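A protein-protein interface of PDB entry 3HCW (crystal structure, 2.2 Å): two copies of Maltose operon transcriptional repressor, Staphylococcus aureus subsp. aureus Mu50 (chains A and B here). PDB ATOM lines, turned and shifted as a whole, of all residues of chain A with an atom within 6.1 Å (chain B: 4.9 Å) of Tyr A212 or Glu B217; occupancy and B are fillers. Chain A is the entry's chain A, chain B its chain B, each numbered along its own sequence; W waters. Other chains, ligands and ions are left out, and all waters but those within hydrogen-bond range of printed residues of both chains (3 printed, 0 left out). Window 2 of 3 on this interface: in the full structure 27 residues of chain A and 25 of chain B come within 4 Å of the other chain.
The backbone NH of Ile B218 sits at hydrogen-bond distance from the side-chain hydroxyl of Tyr A212 (3.0 Å). OG of Ser B237 lies within hydrogen-bond range of O of Leu A208 (3.3 Å).
N of Glu B217 sits at hydrogen-bond distance from OD2 of Asp B221 (2.9 Å). OE2 of Glu B217 is in salt-bridge range of NZ of Lys B220, 3.9 Å away. The backbone carbonyl oxygen (O) of Glu B217 is in hydrogen-bond range of the backbone NH (N) of Val B222 (3.3 Å).
Among the printed residues, merely in contact across the chains: Ser A209 with Ser B237 (3.6 Å), Tyr A212 with Tyr B212 (3.7 Å), Tyr A212 with Glu B217 (3.5 Å), Tyr A212 with Ser B237 (3.9 Å), Tyr A212 with Pro B238 (3.6 Å), Ser A237 with Tyr B212 (3.7 Å) and Ser A237 with Ser B237 (3.8 Å).
Tyr A212 touches five residues of chain B. Of chain A, only Tyr A212 (3.5 Å) comes within 4 Å of Glu B217. Printed residues of chain B within 4 Å of Leu A208: Ser B237. Printed residues of chain A within 4 Å of Ser B237: Leu A208, Ser A209, Tyr A212 and Ser A237. Lys B220 touches none of the printed residues of chain A. Asp B221 touches none of the printed residues of chain A. The nearest residue of chain A that does not touch Glu B217 is Asn A215 (4.4 Å). The nearest printed residue of chain A that does not touch Tyr B212 is Ile A216 (4.2 Å).
Of the 11 printed residues of chain A, 4 touch a printed residue of chain B. Printed residues of chain A that touch a printed residue of chain B: Leu A208, Ser A209, Tyr A212 and Ser A237. Hydrophobic or aromatic side chains of chain A that line the printed part of chain B: Tyr A212. Hydrophobic or aromatic side chains of chain B within 4 Å of the printed part of chain A: Tyr B212, Ile B218 and Pro B238. Among the printed residues, no Asp or Glu carboxylate lies within 4 Å of a Lys or Arg side-chain nitrogen of the other chain.
Tyr B212 touches its own counterpart, Tyr A212. Tyr A212 touches Ser B237, and with the chains exchanged Ser A237 touches Tyr B212. Ser A237 touches its own counterpart, Ser B237.
Water W3 bridges OH of Tyr A212 (2.6 Å) and O of Ile B216 (2.9 Å). Water W1 bridges the backbone carbonyl oxygen (O) of Ile A216 (2.7 Å) and the side-chain hydroxyl (OH) of Tyr B212 (2.7 Å). Water W2 lies within hydrogen-bond range of O of Leu A208 (2.8 Å), O of Ser A237 (2.9 Å) and OG of Ser B237 (3.5 Å).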
ATOM      1  N   ILE A 207     -12.560   3.823  30.783  1.00  0.00           N
ATOM      2  CA  ILE A 207     -13.703   4.128  29.922  1.00  0.00           C
ATOM      3  C   ILE A 207     -13.362   5.233  28.902  1.00  0.00           C
ATOM      4  O   ILE A 207     -13.621   5.069  27.717  1.00  0.00           O
ATOM      5  CB  ILE A 207     -14.979   4.556  30.730  1.00  0.00           C
ATOM      6  CG1 ILE A 207     -15.281   3.626  31.922  1.00  0.00           C
ATOM      7  CG2 ILE A 207     -16.198   4.678  29.805  1.00  0.00           C
ATOM      8  CD1 ILE A 207     -15.669   2.193  31.569  1.00  0.00           C
ATOM      9  N   LEU A 208     -12.781   6.342  29.370  1.00  0.00           N
ATOM     10  CA  LEU A 208     -12.435   7.476  28.500  1.00  0.00           C
ATOM     11  C   LEU A 208     -11.451   7.059  27.414  1.00  0.00           C
ATOM     12  O   LEU A 208     -11.525   7.545  26.290  1.00  0.00           O
ATOM     13  CB  LEU A 208     -11.866   8.654  29.314  1.00  0.00           C
ATOM     14  CG  LEU A 208     -12.747   9.195  30.446  1.00  0.00           C
ATOM     15  CD1 LEU A 208     -12.014  10.198  31.323  1.00  0.00           C
ATOM     16  CD2 LEU A 208     -14.045   9.768  29.933  1.00  0.00           C
ATOM     17  N   SER A 209     -10.556   6.131  27.761  1.00  0.00           N
ATOM     18  CA  SER A 209      -9.546   5.618  26.843  1.00  0.00           C
ATOM     19  C   SER A 209     -10.190   4.838  25.707  1.00  0.00           C
ATOM     20  O   SER A 209      -9.811   5.006  24.545  1.00  0.00           O
ATOM     21  CB  SER A 209      -8.551   4.742  27.599  1.00  0.00           C
ATOM     22  OG  SER A 209      -7.453   4.399  26.769  1.00  0.00           O
ATOM     23  N   VAL A 210     -11.183   4.017  26.045  1.00  0.00           N
ATOM     24  CA  VAL A 210     -11.910   3.237  25.053  1.00  0.00           C
ATOM     25  C   VAL A 210     -12.771   4.173  24.194  1.00  0.00           C
ATOM     26  O   VAL A 210     -12.804   4.047  22.969  1.00  0.00           O
ATOM     27  CB  VAL A 210     -12.720   2.088  25.732  1.00  0.00           C
ATOM     28  CG1 VAL A 210     -13.787   1.522  24.809  1.00  0.00           C
ATOM     29  CG2 VAL A 210     -11.762   0.964  26.204  1.00  0.00           C
ATOM     30  N   LEU A 211     -13.414   5.145  24.841  1.00  0.00           N
ATOM     31  CA  LEU A 211     -14.211   6.175  24.149  1.00  0.00           C
ATOM     32  C   LEU A 211     -13.365   6.994  23.165  1.00  0.00           C
ATOM     33  O   LEU A 211     -13.843   7.356  22.091  1.00  0.00           O
ATOM     34  CB  LEU A 211     -14.924   7.092  25.163  1.00  0.00           C
ATOM     35  CG  LEU A 211     -16.359   6.853  25.633  1.00  0.00           C
ATOM     36  CD1 LEU A 211     -16.809   5.389  25.610  1.00  0.00           C
ATOM     37  CD2 LEU A 211     -16.581   7.459  27.002  1.00  0.00           C
ATOM     38  N   TYR A 212     -12.109   7.253  23.523  1.00  0.00           N
ATOM     39  CA  TYR A 212     -11.159   7.901  22.616  1.00  0.00           C
ATOM     40  C   TYR A 212     -10.899   7.012  21.403  1.00  0.00           C
ATOM     41  O   TYR A 212     -10.953   7.481  20.251  1.00  0.00           O
ATOM     42  CB  TYR A 212      -9.842   8.212  23.338  1.00  0.00           C
ATOM     43  CG  TYR A 212      -8.923   9.142  22.576  1.00  0.00           C
ATOM     44  CD1 TYR A 212      -8.987  10.523  22.766  1.00  0.00           C
ATOM     45  CD2 TYR A 212      -7.981   8.646  21.664  1.00  0.00           C
ATOM     46  CE1 TYR A 212      -8.143  11.392  22.070  1.00  0.00           C
ATOM     47  CE2 TYR A 212      -7.145   9.512  20.951  1.00  0.00           C
ATOM     48  CZ  TYR A 212      -7.225  10.883  21.171  1.00  0.00           C
ATOM     49  OH  TYR A 212      -6.391  11.745  20.485  1.00  0.00           O
ATOM     50  N   GLU A 213     -10.667   5.725  21.669  1.00  0.00           N
ATOM     51  CA  GLU A 213     -10.366   4.745  20.625  1.00  0.00           C
ATOM     52  C   GLU A 213     -11.495   4.622  19.593  1.00  0.00           C
ATOM     53  O   GLU A 213     -11.236   4.410  18.419  1.00  0.00           O
ATOM     54  CB  GLU A 213     -10.008   3.385  21.241  1.00  0.00           C
ATOM     55  CG  GLU A 213      -9.505   2.339  20.239  1.00  0.00           C
ATOM     56  CD  GLU A 213      -8.764   1.169  20.883  1.00  0.00           C
ATOM     57  OE1 GLU A 213      -7.862   0.610  20.223  1.00  0.00           O
ATOM     58  OE2 GLU A 213      -9.081   0.800  22.035  1.00  0.00           O
ATOM     59  N   LEU A 214     -12.735   4.797  20.040  1.00  0.00           N
ATOM     60  CA  LEU A 214     -13.909   4.651  19.199  1.00  0.00           C
ATOM     61  C   LEU A 214     -14.394   5.963  18.616  1.00  0.00           C
ATOM     62  O   LEU A 214     -15.415   5.989  17.924  1.00  0.00           O
ATOM     63  CB  LEU A 214     -15.043   4.003  19.997  1.00  0.00           C
ATOM     64  CG  LEU A 214     -14.831   2.549  20.441  1.00  0.00           C
ATOM     65  CD1 LEU A 214     -16.024   2.092  21.246  1.00  0.00           C
ATOM     66  CD2 LEU A 214     -14.624   1.639  19.239  1.00  0.00           C
ATOM     67  N   ASN A 215     -13.645   7.034  18.890  1.00  0.00           N
ATOM     68  CA  ASN A 215     -13.967   8.397  18.471  1.00  0.00           C
ATOM     69  C   ASN A 215     -15.330   8.886  18.950  1.00  0.00           C
ATOM     70  O   ASN A 215     -16.014   9.625  18.251  1.00  0.00           O
ATOM     71  CB  ASN A 215     -13.810   8.570  16.953  1.00  0.00           C
ATOM     72  CG  ASN A 215     -13.591  10.025  16.545  1.00  0.00           C
ATOM     73  OD1 ASN A 215     -14.121  10.477  15.528  1.00  0.00           O
ATOM     74  ND2 ASN A 215     -12.818  10.764  17.342  1.00  0.00           N
ATOM     75  N   ILE A 216     -15.706   8.465  20.154  1.00  0.00           N
ATOM     76  CA  ILE A 216     -16.931   8.918  20.808  1.00  0.00           C
ATOM     77  C   ILE A 216     -16.571  10.139  21.667  1.00  0.00           C
ATOM     78  O   ILE A 216     -16.016   9.999  22.763  1.00  0.00           O
ATOM     79  CB  ILE A 216     -17.550   7.795  21.658  1.00  0.00           C
ATOM     80  CG1 ILE A 216     -17.821   6.562  20.792  1.00  0.00           C
ATOM     81  CG2 ILE A 216     -18.827   8.275  22.322  1.00  0.00           C
ATOM     82  CD1 ILE A 216     -18.187   5.321  21.573  1.00  0.00           C
ATOM     83  N   SER A 237      -9.022  13.526  29.844  1.00  0.00           N
ATOM     84  CA  SER A 237      -9.372  13.955  28.504  1.00  0.00           C
ATOM     85  C   SER A 237     -10.829  13.574  28.221  1.00  0.00           C
ATOM     86  O   SER A 237     -11.110  12.404  27.939  1.00  0.00           O
ATOM     87  CB  SER A 237      -8.446  13.296  27.465  1.00  0.00           C
ATOM     88  OG  SER A 237      -7.084  13.679  27.662  1.00  0.00           O
ATOM     89  N   TYR B 212      -6.790  17.055  23.546  1.00  0.00           N
ATOM     90  CA  TYR B 212      -8.196  16.649  23.409  1.00  0.00           C
ATOM     91  C   TYR B 212      -9.096  17.877  23.188  1.00  0.00           C
ATOM     92  O   TYR B 212      -9.935  17.887  22.285  1.00  0.00           O
ATOM     93  CB  TYR B 212      -8.665  15.866  24.649  1.00  0.00           C
ATOM     94  CG  TYR B 212     -10.011  15.185  24.478  1.00  0.00           C
ATOM     95  CD1 TYR B 212     -10.079  13.824  24.149  1.00  0.00           C
ATOM     96  CD2 TYR B 212     -11.211  15.884  24.657  1.00  0.00           C
ATOM     97  CE1 TYR B 212     -11.299  13.170  23.995  1.00  0.00           C
ATOM     98  CE2 TYR B 212     -12.455  15.241  24.484  1.00  0.00           C
ATOM     99  CZ  TYR B 212     -12.476  13.877  24.159  1.00  0.00           C
ATOM    100  OH  TYR B 212     -13.649  13.213  23.974  1.00  0.00           O
ATOM    101  N   ASN B 215      -8.811  19.359  19.657  1.00  0.00           N
ATOM    102  CA  ASN B 215      -9.122  18.393  18.591  1.00  0.00           C
ATOM    103  C   ASN B 215      -7.917  17.918  17.784  1.00  0.00           C
ATOM    104  O   ASN B 215      -8.006  17.675  16.582  1.00  0.00           O
ATOM    105  CB  ASN B 215     -10.225  18.911  17.664  1.00  0.00           C
ATOM    106  CG  ASN B 215     -11.594  18.499  18.124  1.00  0.00           C
ATOM    107  OD1 ASN B 215     -12.280  19.252  18.812  1.00  0.00           O
ATOM    108  ND2 ASN B 215     -11.993  17.283  17.768  1.00  0.00           N
ATOM    109  N   ILE B 216      -6.793  17.781  18.471  1.00  0.00           N
ATOM    110  CA  ILE B 216      -5.563  17.332  17.866  1.00  0.00           C
ATOM    111  C   ILE B 216      -5.438  15.844  18.207  1.00  0.00           C
ATOM    112  O   ILE B 216      -5.015  15.487  19.307  1.00  0.00           O
ATOM    113  CB  ILE B 216      -4.363  18.175  18.395  1.00  0.00           C
ATOM    114  CG1 ILE B 216      -4.631  19.672  18.201  1.00  0.00           C
ATOM    115  CG2 ILE B 216      -3.090  17.803  17.676  1.00  0.00           C
ATOM    116  CD1 ILE B 216      -3.595  20.592  18.824  1.00  0.00           C
ATOM    117  N   GLU B 217      -5.851  14.981  17.277  1.00  0.00           N
ATOM    118  CA  GLU B 217      -5.897  13.541  17.548  1.00  0.00           C
ATOM    119  C   GLU B 217      -4.555  12.831  17.433  1.00  0.00           C
ATOM    120  O   GLU B 217      -3.668  13.250  16.693  1.00  0.00           O
ATOM    121  CB  GLU B 217      -6.983  12.810  16.749  1.00  0.00           C
ATOM    122  CG  GLU B 217      -7.092  13.141  15.282  1.00  0.00           C
ATOM    123  CD  GLU B 217      -8.398  12.627  14.678  1.00  0.00           C
ATOM    124  OE1 GLU B 217      -9.012  11.703  15.267  1.00  0.00           O
ATOM    125  OE2 GLU B 217      -8.812  13.148  13.618  1.00  0.00           O
ATOM    126  N   ILE B 218      -4.435  11.757  18.206  1.00  0.00           N
ATOM    127  CA  ILE B 218      -3.205  11.013  18.390  1.00  0.00           C
ATOM    128  C   ILE B 218      -3.522   9.554  18.053  1.00  0.00           C
ATOM    129  O   ILE B 218      -4.522   9.017  18.525  1.00  0.00           O
ATOM    130  CB  ILE B 218      -2.716  11.149  19.867  1.00  0.00           C
ATOM    131  CG1 ILE B 218      -2.521  12.624  20.229  1.00  0.00           C
ATOM    132  CG2 ILE B 218      -1.404  10.369  20.130  1.00  0.00           C
ATOM    133  CD1 ILE B 218      -2.515  12.899  21.710  1.00  0.00           C
ATOM    134  N   PRO B 219      -2.691   8.910  17.215  1.00  0.00           N
ATOM    135  CA  PRO B 219      -1.471   9.431  16.589  1.00  0.00           C
ATOM    136  C   PRO B 219      -1.676  10.047  15.184  1.00  0.00           C
ATOM    137  O   PRO B 219      -0.698  10.230  14.461  1.00  0.00           O
ATOM    138  CB  PRO B 219      -0.608   8.177  16.490  1.00  0.00           C
ATOM    139  CG  PRO B 219      -1.634   7.094  16.144  1.00  0.00           C
ATOM    140  CD  PRO B 219      -2.929   7.503  16.838  1.00  0.00           C
ATOM    141  N   LYS B 220      -2.918  10.363  14.812  1.00  0.00           N
ATOM    142  CA  LYS B 220      -3.215  10.893  13.472  1.00  0.00           C
ATOM    143  C   LYS B 220      -2.566  12.252  13.189  1.00  0.00           C
ATOM    144  O   LYS B 220      -1.833  12.379  12.219  1.00  0.00           O
ATOM    145  CB  LYS B 220      -4.721  10.965  13.226  1.00  0.00           C
ATOM    146  CG  LYS B 220      -5.104  11.135  11.763  1.00  0.00           C
ATOM    147  CD  LYS B 220      -6.594  11.362  11.617  1.00  0.00           C
ATOM    148  CE  LYS B 220      -6.978  11.585  10.167  1.00  0.00           C
ATOM    149  NZ  LYS B 220      -8.449  11.777  10.035  1.00  0.00           N
ATOM    150  N   ASP B 221      -2.824  13.248  14.036  1.00  0.00           N
ATOM    151  CA  ASP B 221      -2.222  14.583  13.877  1.00  0.00           C
ATOM    152  C   ASP B 221      -0.812  14.691  14.465  1.00  0.00           C
ATOM    153  O   ASP B 221       0.081  15.234  13.815  1.00  0.00           O
ATOM    154  CB  ASP B 221      -3.118  15.676  14.474  1.00  0.00           C
ATOM    155  CG  ASP B 221      -4.503  15.706  13.854  1.00  0.00           C
ATOM    156  OD1 ASP B 221      -4.640  15.417  12.643  1.00  0.00           O
ATOM    157  OD2 ASP B 221      -5.460  16.026  14.585  1.00  0.00           O
ATOM    158  N   VAL B 222      -0.641  14.232  15.712  1.00  0.00           N
ATOM    159  CA  VAL B 222       0.679  14.156  16.352  1.00  0.00           C
ATOM    160  C   VAL B 222       0.862  12.849  17.096  1.00  0.00           C
ATOM    161  O   VAL B 222      -0.082  12.326  17.702  1.00  0.00           O
ATOM    162  CB  VAL B 222       0.965  15.298  17.368  1.00  0.00           C
ATOM    163  CG1 VAL B 222       1.396  16.558  16.660  1.00  0.00           C
ATOM    164  CG2 VAL B 222      -0.220  15.537  18.323  1.00  0.00           C
ATOM    165  N   SER B 237      -5.550   8.611  27.169  1.00  0.00           N
ATOM    166  CA  SER B 237      -6.345   8.838  25.966  1.00  0.00           C
ATOM    167  C   SER B 237      -5.488   9.467  24.846  1.00  0.00           C
ATOM    168  O   SER B 237      -5.368  10.701  24.779  1.00  0.00           O
ATOM    169  CB  SER B 237      -7.544   9.753  26.282  1.00  0.00           C
ATOM    170  OG  SER B 237      -8.618   9.069  26.917  1.00  0.00           O
ATOM    171  N   PRO B 238      -4.890   8.638  23.957  1.00  0.00           N
ATOM    172  CA  PRO B 238      -4.876   7.166  23.850  1.00  0.00           C
ATOM    173  C   PRO B 238      -3.715   6.545  24.664  1.00  0.00           C
ATOM    174  O   PRO B 238      -2.862   7.283  25.171  1.00  0.00           O
ATOM    175  CB  PRO B 238      -4.650   6.957  22.348  1.00  0.00           C
ATOM    176  CG  PRO B 238      -3.681   8.052  22.009  1.00  0.00           C
ATOM    177  CD  PRO B 238      -4.111   9.250  22.859  1.00  0.00           C
HETATM  178  O   HOH W   1     -13.555  10.506  23.724  1.00  0.00           O
HETATM  179  O   HOH W   2     -11.714  10.331  26.028  1.00  0.00           O
HETATM  180  O   HOH W   3      -6.191  14.078  21.499  1.00  0.00           O
